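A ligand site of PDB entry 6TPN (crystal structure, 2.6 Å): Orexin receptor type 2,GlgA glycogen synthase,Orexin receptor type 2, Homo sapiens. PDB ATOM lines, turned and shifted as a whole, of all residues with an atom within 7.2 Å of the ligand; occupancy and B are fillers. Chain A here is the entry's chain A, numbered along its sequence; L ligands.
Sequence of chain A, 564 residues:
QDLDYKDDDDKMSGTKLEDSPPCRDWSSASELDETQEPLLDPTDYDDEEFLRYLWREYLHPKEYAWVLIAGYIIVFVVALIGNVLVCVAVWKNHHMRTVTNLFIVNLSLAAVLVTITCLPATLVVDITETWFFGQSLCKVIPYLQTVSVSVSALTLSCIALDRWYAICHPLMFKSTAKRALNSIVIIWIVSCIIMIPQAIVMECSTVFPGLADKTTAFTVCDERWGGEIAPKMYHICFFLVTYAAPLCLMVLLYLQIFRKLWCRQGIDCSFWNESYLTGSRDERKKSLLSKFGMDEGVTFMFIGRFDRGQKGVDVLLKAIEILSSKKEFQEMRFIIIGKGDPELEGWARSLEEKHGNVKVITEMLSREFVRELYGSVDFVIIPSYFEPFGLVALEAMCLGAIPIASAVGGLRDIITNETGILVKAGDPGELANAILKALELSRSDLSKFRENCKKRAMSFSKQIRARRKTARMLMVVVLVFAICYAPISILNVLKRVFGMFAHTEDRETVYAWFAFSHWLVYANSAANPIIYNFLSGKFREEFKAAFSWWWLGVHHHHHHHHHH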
ATOM      1  N   PHE A 103     -24.188  17.127  -8.767  1.00  0.00           N
ATOM      2  CA  PHE A 103     -23.759  15.995  -9.570  1.00  0.00           C
ATOM      3  C   PHE A 103     -22.940  15.004  -8.744  1.00  0.00           C
ATOM      4  O   PHE A 103     -23.122  13.787  -8.874  1.00  0.00           O
ATOM      5  CB  PHE A 103     -22.944  16.485 -10.759  1.00  0.00           C
ATOM      6  CG  PHE A 103     -23.769  16.895 -11.939  1.00  0.00           C
ATOM      7  CD1 PHE A 103     -24.795  16.083 -12.411  1.00  0.00           C
ATOM      8  CD2 PHE A 103     -23.521  18.097 -12.579  1.00  0.00           C
ATOM      9  CE1 PHE A 103     -25.552  16.464 -13.493  1.00  0.00           C
ATOM     10  CE2 PHE A 103     -24.278  18.482 -13.670  1.00  0.00           C
ATOM     11  CZ  PHE A 103     -25.294  17.667 -14.132  1.00  0.00           C
ATOM     12  N   SER A 150     -23.002   3.343 -16.181  1.00  0.00           N
ATOM     13  CA  SER A 150     -23.433   4.320 -17.171  1.00  0.00           C
ATOM     14  C   SER A 150     -23.745   5.663 -16.519  1.00  0.00           C
ATOM     15  O   SER A 150     -23.374   6.723 -17.054  1.00  0.00           O
ATOM     16  CB  SER A 150     -24.650   3.801 -17.932  1.00  0.00           C
ATOM     17  OG  SER A 150     -25.071   4.744 -18.911  1.00  0.00           O
ATOM     18  N   LEU A 154     -21.654   9.277 -17.365  1.00  0.00           N
ATOM     19  CA  LEU A 154     -22.388  10.417 -17.890  1.00  0.00           C
ATOM     20  C   LEU A 154     -22.434  11.582 -16.900  1.00  0.00           C
ATOM     21  O   LEU A 154     -22.502  12.744 -17.329  1.00  0.00           O
ATOM     22  CB  LEU A 154     -23.801   9.991 -18.279  1.00  0.00           C
ATOM     23  CG  LEU A 154     -23.865   8.913 -19.359  1.00  0.00           C
ATOM     24  CD1 LEU A 154     -25.282   8.408 -19.532  1.00  0.00           C
ATOM     25  CD2 LEU A 154     -23.318   9.443 -20.679  1.00  0.00           C
ATOM     26  N   SER A 157     -19.084  13.290 -17.118  1.00  0.00           N
ATOM     27  CA  SER A 157     -18.991  14.083 -18.343  1.00  0.00           C
ATOM     28  C   SER A 157     -19.783  15.373 -18.223  1.00  0.00           C
ATOM     29  O   SER A 157     -19.362  16.422 -18.750  1.00  0.00           O
ATOM     30  CB  SER A 157     -19.480  13.264 -19.540  1.00  0.00           C
ATOM     31  OG  SER A 157     -18.721  12.064 -19.684  1.00  0.00           O
ATOM     32  N   CYS A 158     -20.936  15.335 -17.548  1.00  0.00           N
ATOM     33  CA  CYS A 158     -21.727  16.553 -17.366  1.00  0.00           C
ATOM     34  C   CYS A 158     -21.044  17.537 -16.428  1.00  0.00           C
ATOM     35  O   CYS A 158     -21.264  18.739 -16.543  1.00  0.00           O
ATOM     36  CB  CYS A 158     -23.125  16.203 -16.838  1.00  0.00           C
ATOM     37  SG  CYS A 158     -24.259  15.563 -18.097  1.00  0.00           S
ATOM     38  N   ILE A 159     -20.227  17.038 -15.497  1.00  0.00           N
ATOM     39  CA  ILE A 159     -19.458  17.926 -14.640  1.00  0.00           C
ATOM     40  C   ILE A 159     -18.406  18.664 -15.451  1.00  0.00           C
ATOM     41  O   ILE A 159     -18.244  19.883 -15.331  1.00  0.00           O
ATOM     42  CB  ILE A 159     -18.839  17.141 -13.469  1.00  0.00           C
ATOM     43  CG1 ILE A 159     -19.927  16.670 -12.511  1.00  0.00           C
ATOM     44  CG2 ILE A 159     -17.825  18.005 -12.729  1.00  0.00           C
ATOM     45  CD1 ILE A 159     -19.420  15.754 -11.437  1.00  0.00           C
ATOM     46  N   ALA A 160     -17.689  17.931 -16.309  1.00  0.00           N
ATOM     47  CA  ALA A 160     -16.730  18.576 -17.205  1.00  0.00           C
ATOM     48  C   ALA A 160     -17.432  19.521 -18.169  1.00  0.00           C
ATOM     49  O   ALA A 160     -16.931  20.621 -18.447  1.00  0.00           O
ATOM     50  CB  ALA A 160     -15.944  17.501 -17.970  1.00  0.00           C
ATOM     51  N   LEU A 161     -18.590  19.108 -18.694  1.00  0.00           N
ATOM     52  CA  LEU A 161     -19.350  19.951 -19.608  1.00  0.00           C
ATOM     53  C   LEU A 161     -19.761  21.244 -18.911  1.00  0.00           C
ATOM     54  O   LEU A 161     -19.524  22.350 -19.414  1.00  0.00           O
ATOM     55  CB  LEU A 161     -20.577  19.192 -20.110  1.00  0.00           C
ATOM     56  CG  LEU A 161     -20.950  19.284 -21.580  1.00  0.00           C
ATOM     57  CD1 LEU A 161     -19.838  18.707 -22.442  1.00  0.00           C
ATOM     58  CD2 LEU A 161     -22.256  18.560 -21.841  1.00  0.00           C
ATOM     59  N   ASP A 162     -20.378  21.125 -17.735  1.00  0.00           N
ATOM     60  CA  ASP A 162     -20.817  22.306 -16.991  1.00  0.00           C
ATOM     61  C   ASP A 162     -19.640  23.217 -16.673  1.00  0.00           C
ATOM     62  O   ASP A 162     -19.751  24.449 -16.766  1.00  0.00           O
ATOM     63  CB  ASP A 162     -21.577  21.888 -15.724  1.00  0.00           C
ATOM     64  CG  ASP A 162     -21.723  23.008 -14.709  1.00  0.00           C
ATOM     65  OD1 ASP A 162     -22.400  24.018 -15.011  1.00  0.00           O
ATOM     66  OD2 ASP A 162     -21.146  22.905 -13.605  1.00  0.00           O
ATOM     67  N   TYR A 165     -18.452  25.089 -19.975  1.00  0.00           N
ATOM     68  CA  TYR A 165     -19.359  26.156 -20.359  1.00  0.00           C
ATOM     69  C   TYR A 165     -19.305  27.345 -19.401  1.00  0.00           C
ATOM     70  O   TYR A 165     -19.692  28.449 -19.793  1.00  0.00           O
ATOM     71  CB  TYR A 165     -20.798  25.635 -20.453  1.00  0.00           C
ATOM     72  CG  TYR A 165     -21.152  25.071 -21.807  1.00  0.00           C
ATOM     73  CD1 TYR A 165     -20.732  23.806 -22.190  1.00  0.00           C
ATOM     74  CD2 TYR A 165     -21.919  25.813 -22.700  1.00  0.00           C
ATOM     75  CE1 TYR A 165     -21.061  23.292 -23.432  1.00  0.00           C
ATOM     76  CE2 TYR A 165     -22.258  25.299 -23.943  1.00  0.00           C
ATOM     77  CZ  TYR A 165     -21.819  24.038 -24.304  1.00  0.00           C
ATOM     78  OH  TYR A 165     -22.159  23.533 -25.544  1.00  0.00           O
ATOM     79  N   SER A 175     -25.245  27.602 -14.647  1.00  0.00           N
ATOM     80  CA  SER A 175     -26.347  26.665 -14.541  1.00  0.00           C
ATOM     81  C   SER A 175     -27.019  26.774 -13.167  1.00  0.00           C
ATOM     82  O   SER A 175     -26.440  27.283 -12.204  1.00  0.00           O
ATOM     83  CB  SER A 175     -25.857  25.236 -14.765  1.00  0.00           C
ATOM     84  OG  SER A 175     -25.247  25.101 -16.033  1.00  0.00           O
ATOM     85  N   ARG A 179     -31.768  22.915 -13.363  1.00  0.00           N
ATOM     86  CA  ARG A 179     -31.215  22.342 -14.583  1.00  0.00           C
ATOM     87  C   ARG A 179     -30.281  21.170 -14.295  1.00  0.00           C
ATOM     88  O   ARG A 179     -30.150  20.274 -15.123  1.00  0.00           O
ATOM     89  CB  ARG A 179     -30.506  23.428 -15.385  1.00  0.00           C
ATOM     90  CG  ARG A 179     -30.022  22.983 -16.755  1.00  0.00           C
ATOM     91  CD  ARG A 179     -29.116  24.029 -17.398  1.00  0.00           C
ATOM     92  NE  ARG A 179     -28.465  23.494 -18.593  1.00  0.00           N
ATOM     93  CZ  ARG A 179     -28.956  23.589 -19.823  1.00  0.00           C
ATOM     94  NH1 ARG A 179     -30.113  24.206 -20.021  1.00  0.00           N
ATOM     95  NH2 ARG A 179     -28.302  23.073 -20.844  1.00  0.00           N
ATOM     96  N   ALA A 180     -29.641  21.162 -13.117  1.00  0.00           N
ATOM     97  CA  ALA A 180     -28.752  20.063 -12.765  1.00  0.00           C
ATOM     98  C   ALA A 180     -29.522  18.813 -12.352  1.00  0.00           C
ATOM     99  O   ALA A 180     -29.072  17.699 -12.613  1.00  0.00           O
ATOM    100  CB  ALA A 180     -27.805  20.486 -11.642  1.00  0.00           C
ATOM    101  N   ASN A 182     -32.702  18.070 -13.428  1.00  0.00           N
ATOM    102  CA  ASN A 182     -33.352  17.534 -14.612  1.00  0.00           C
ATOM    103  C   ASN A 182     -32.373  16.781 -15.501  1.00  0.00           C
ATOM    104  O   ASN A 182     -32.746  15.774 -16.125  1.00  0.00           O
ATOM    105  CB  ASN A 182     -34.036  18.644 -15.397  1.00  0.00           C
ATOM    106  CG  ASN A 182     -35.400  18.989 -14.835  1.00  0.00           C
ATOM    107  OD1 ASN A 182     -35.522  19.848 -13.955  1.00  0.00           O
ATOM    108  ND2 ASN A 182     -36.430  18.319 -15.324  1.00  0.00           N
ATOM    109  N   SER A 183     -31.126  17.242 -15.578  1.00  0.00           N
ATOM    110  CA  SER A 183     -30.102  16.462 -16.275  1.00  0.00           C
ATOM    111  C   SER A 183     -29.791  15.177 -15.523  1.00  0.00           C
ATOM    112  O   SER A 183     -29.453  14.167 -16.131  1.00  0.00           O
ATOM    113  CB  SER A 183     -28.845  17.302 -16.451  1.00  0.00           C
ATOM    114  OG  SER A 183     -29.143  18.572 -16.987  1.00  0.00           O
ATOM    115  N   ILE A 184     -29.908  15.210 -14.192  1.00  0.00           N
ATOM    116  CA  ILE A 184     -29.663  14.021 -13.390  1.00  0.00           C
ATOM    117  C   ILE A 184     -30.769  12.991 -13.618  1.00  0.00           C
ATOM    118  O   ILE A 184     -30.501  11.790 -13.733  1.00  0.00           O
ATOM    119  CB  ILE A 184     -29.537  14.395 -11.903  1.00  0.00           C
ATOM    120  CG1 ILE A 184     -28.103  14.865 -11.615  1.00  0.00           C
ATOM    121  CG2 ILE A 184     -29.958  13.247 -10.998  1.00  0.00           C
ATOM    122  CD1 ILE A 184     -27.943  15.538 -10.274  1.00  0.00           C
ATOM    123  N   ILE A 186     -32.497  12.701 -16.333  1.00  0.00           N
ATOM    124  CA  ILE A 186     -32.331  12.197 -17.697  1.00  0.00           C
ATOM    125  C   ILE A 186     -31.220  11.154 -17.753  1.00  0.00           C
ATOM    126  O   ILE A 186     -31.339  10.149 -18.475  1.00  0.00           O
ATOM    127  CB  ILE A 186     -32.080  13.367 -18.662  1.00  0.00           C
ATOM    128  CG1 ILE A 186     -33.356  14.189 -18.828  1.00  0.00           C
ATOM    129  CG2 ILE A 186     -31.585  12.862 -20.009  1.00  0.00           C
ATOM    130  CD1 ILE A 186     -33.113  15.528 -19.435  1.00  0.00           C
ATOM    131  N   ILE A 187     -30.143  11.377 -17.006  1.00  0.00           N
ATOM    132  CA  ILE A 187     -29.038  10.423 -16.980  1.00  0.00           C
ATOM    133  C   ILE A 187     -29.513   9.045 -16.549  1.00  0.00           C
ATOM    134  O   ILE A 187     -29.116   8.020 -17.129  1.00  0.00           O
ATOM    135  CB  ILE A 187     -27.907  10.945 -16.074  1.00  0.00           C
ATOM    136  CG1 ILE A 187     -27.175  12.107 -16.747  1.00  0.00           C
ATOM    137  CG2 ILE A 187     -26.947   9.823 -15.706  1.00  0.00           C
ATOM    138  CD1 ILE A 187     -26.336  12.936 -15.791  1.00  0.00           C
ATOM    139  N   VAL A 190     -31.694   7.516 -19.365  1.00  0.00           N
ATOM    140  CA  VAL A 190     -30.877   7.049 -20.482  1.00  0.00           C
ATOM    141  C   VAL A 190     -30.162   5.747 -20.115  1.00  0.00           C
ATOM    142  O   VAL A 190     -30.160   4.784 -20.884  1.00  0.00           O
ATOM    143  CB  VAL A 190     -29.871   8.136 -20.910  1.00  0.00           C
ATOM    144  CG1 VAL A 190     -28.845   7.554 -21.870  1.00  0.00           C
ATOM    145  CG2 VAL A 190     -30.602   9.310 -21.540  1.00  0.00           C
ATOM    146  N   SER A 191     -29.541   5.716 -18.934  1.00  0.00           N
ATOM    147  CA  SER A 191     -28.811   4.524 -18.511  1.00  0.00           C
ATOM    148  C   SER A 191     -29.732   3.312 -18.404  1.00  0.00           C
ATOM    149  O   SER A 191     -29.378   2.211 -18.820  1.00  0.00           O
ATOM    150  CB  SER A 191     -28.126   4.782 -17.173  1.00  0.00           C
ATOM    151  OG  SER A 191     -27.189   5.836 -17.278  1.00  0.00           O
ATOM    152  N   ILE A 194     -30.491   2.103 -22.114  1.00  0.00           N
ATOM    153  CA  ILE A 194     -29.403   1.558 -22.914  1.00  0.00           C
ATOM    154  C   ILE A 194     -28.836   0.273 -22.324  1.00  0.00           C
ATOM    155  O   ILE A 194     -28.144  -0.469 -23.028  1.00  0.00           O
ATOM    156  CB  ILE A 194     -28.283   2.599 -23.081  1.00  0.00           C
ATOM    157  CG1 ILE A 194     -27.704   2.993 -21.724  1.00  0.00           C
ATOM    158  CG2 ILE A 194     -28.782   3.814 -23.839  1.00  0.00           C
ATOM    159  CD1 ILE A 194     -26.471   3.868 -21.816  1.00  0.00           C
ATOM    160  N   CYS A 237     -19.777  -1.267 -28.161  1.00  0.00           N
ATOM    161  CA  CYS A 237     -20.602  -0.124 -27.815  1.00  0.00           C
ATOM    162  C   CYS A 237     -20.652   0.098 -26.307  1.00  0.00           C
ATOM    163  O   CYS A 237     -20.888   1.226 -25.859  1.00  0.00           O
ATOM    164  CB  CYS A 237     -22.018  -0.309 -28.369  1.00  0.00           C
ATOM    165  SG  CYS A 237     -22.147  -0.266 -30.174  1.00  0.00           S
ATOM    166  N   PHE A 238     -20.361  -0.934 -25.528  1.00  0.00           N
ATOM    167  CA  PHE A 238     -20.338  -0.764 -24.045  1.00  0.00           C
ATOM    168  C   PHE A 238     -19.035  -0.063 -23.676  1.00  0.00           C
ATOM    169  O   PHE A 238     -19.046   0.859 -22.878  1.00  0.00           O
ATOM    170  CB  PHE A 238     -20.454  -2.116 -23.345  1.00  0.00           C
ATOM    171  CG  PHE A 238     -20.588  -2.052 -21.847  1.00  0.00           C
ATOM    172  CD1 PHE A 238     -21.829  -2.091 -21.248  1.00  0.00           C
ATOM    173  CD2 PHE A 238     -19.478  -1.953 -21.034  1.00  0.00           C
ATOM    174  CE1 PHE A 238     -21.949  -2.010 -19.870  1.00  0.00           C
ATOM    175  CE2 PHE A 238     -19.609  -1.872 -19.657  1.00  0.00           C
ATOM    176  CZ  PHE A 238     -20.839  -1.905 -19.076  1.00  0.00           C
ATOM    177  N   LEU A 240     -17.332   1.928 -25.490  1.00  0.00           N
ATOM    178  CA  LEU A 240     -17.334   3.294 -25.989  1.00  0.00           C
ATOM    179  C   LEU A 240     -18.179   4.216 -25.115  1.00  0.00           C
ATOM    180  O   LEU A 240     -17.692   5.240 -24.630  1.00  0.00           O
ATOM    181  CB  LEU A 240     -17.846   3.322 -27.440  1.00  0.00           C
ATOM    182  CG  LEU A 240     -16.917   2.736 -28.498  1.00  0.00           C
ATOM    183  CD1 LEU A 240     -17.683   2.431 -29.768  1.00  0.00           C
ATOM    184  CD2 LEU A 240     -15.771   3.687 -28.777  1.00  0.00           C
ATOM    185  N   VAL A 241     -19.435   3.842 -24.886  1.00  0.00           N
ATOM    186  CA  VAL A 241     -20.353   4.725 -24.163  1.00  0.00           C
ATOM    187  C   VAL A 241     -19.948   4.867 -22.702  1.00  0.00           C
ATOM    188  O   VAL A 241     -20.118   5.942 -22.110  1.00  0.00           O
ATOM    189  CB  VAL A 241     -21.801   4.199 -24.312  1.00  0.00           C
ATOM    190  CG1 VAL A 241     -22.761   4.984 -23.422  1.00  0.00           C
ATOM    191  CG2 VAL A 241     -22.244   4.274 -25.768  1.00  0.00           C
HETATM  192  C1  LIG L   1     -25.566  19.558 -18.963  1.00  0.00           C
HETATM  193  O1  LIG L   1     -26.151  20.470 -18.350  1.00  0.00           O
HETATM  194  O2  LIG L   1     -24.430  19.141 -18.640  1.00  0.00           O
HETATM  195  C2  LIG L   1     -26.253  18.925 -20.147  1.00  0.00           C
HETATM  196  C3  LIG L   1     -27.286  17.936 -19.636  1.00  0.00           C
HETATM  197  C4  LIG L   1     -27.673  16.926 -20.712  1.00  0.00           C
HETATM  198  C5  LIG L   1     -27.793  15.525 -20.122  1.00  0.00           C
HETATM  199  C6  LIG L   1     -26.813  14.569 -20.804  1.00  0.00           C
HETATM  200  C7  LIG L   1     -27.345  13.143 -20.725  1.00  0.00           C
HETATM  201  C8  LIG L   1     -26.627  12.206 -21.700  1.00  0.00           C
HETATM  202  C9  LIG L   1     -27.625  11.728 -22.726  1.00  0.00           C
HETATM  203  C10 LIG L   1     -27.261  10.933 -23.738  1.00  0.00           C
HETATM  204  C11 LIG L   1     -25.827  10.457 -23.878  1.00  0.00           C
HETATM  205  C12 LIG L   1     -25.816   8.943 -23.772  1.00  0.00           C
HETATM  206  C13 LIG L   1     -25.062   8.308 -24.934  1.00  0.00           C
HETATM  207  C14 LIG L   1     -25.414   6.831 -25.067  1.00  0.00           C
HETATM  208  C15 LIG L   1     -25.793   6.503 -26.503  1.00  0.00           C
HETATM  209  C16 LIG L   1     -25.639   5.011 -26.807  1.00  0.00           C
HETATM  210  C17 LIG L   1     -25.023   4.805 -28.182  1.00  0.00           C
HETATM  211  C18 LIG L   1     -24.642   3.350 -28.406  1.00  0.00           C
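The side-chain sulfur of Cys 158 sits at hydrogen-bond distance from an oxygen (O2) of the ligand, 3.6 Å away.
O1 of the ligand lies within salt-bridge range of NE of Arg 179, at 3.8 Å.
OG of Ser 183 sits at hydrogen-bond distance from O of Arg 179, 2.7 Å away.
The backbone carbonyl oxygen (O) of Leu 154 lies within hydrogen-bond range of the side-chain sulfur (SG) of Cys 158.
Residues that only touch the ligand: Ser 183, Val 241, Val 190 and Leu 161.
Hydrophobic or aromatic side chains that line the ligand: Leu 161, Val 190 and Val 241.
The nearest printed residue that does not touch the ligand is Leu 154 (4.01 Å).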
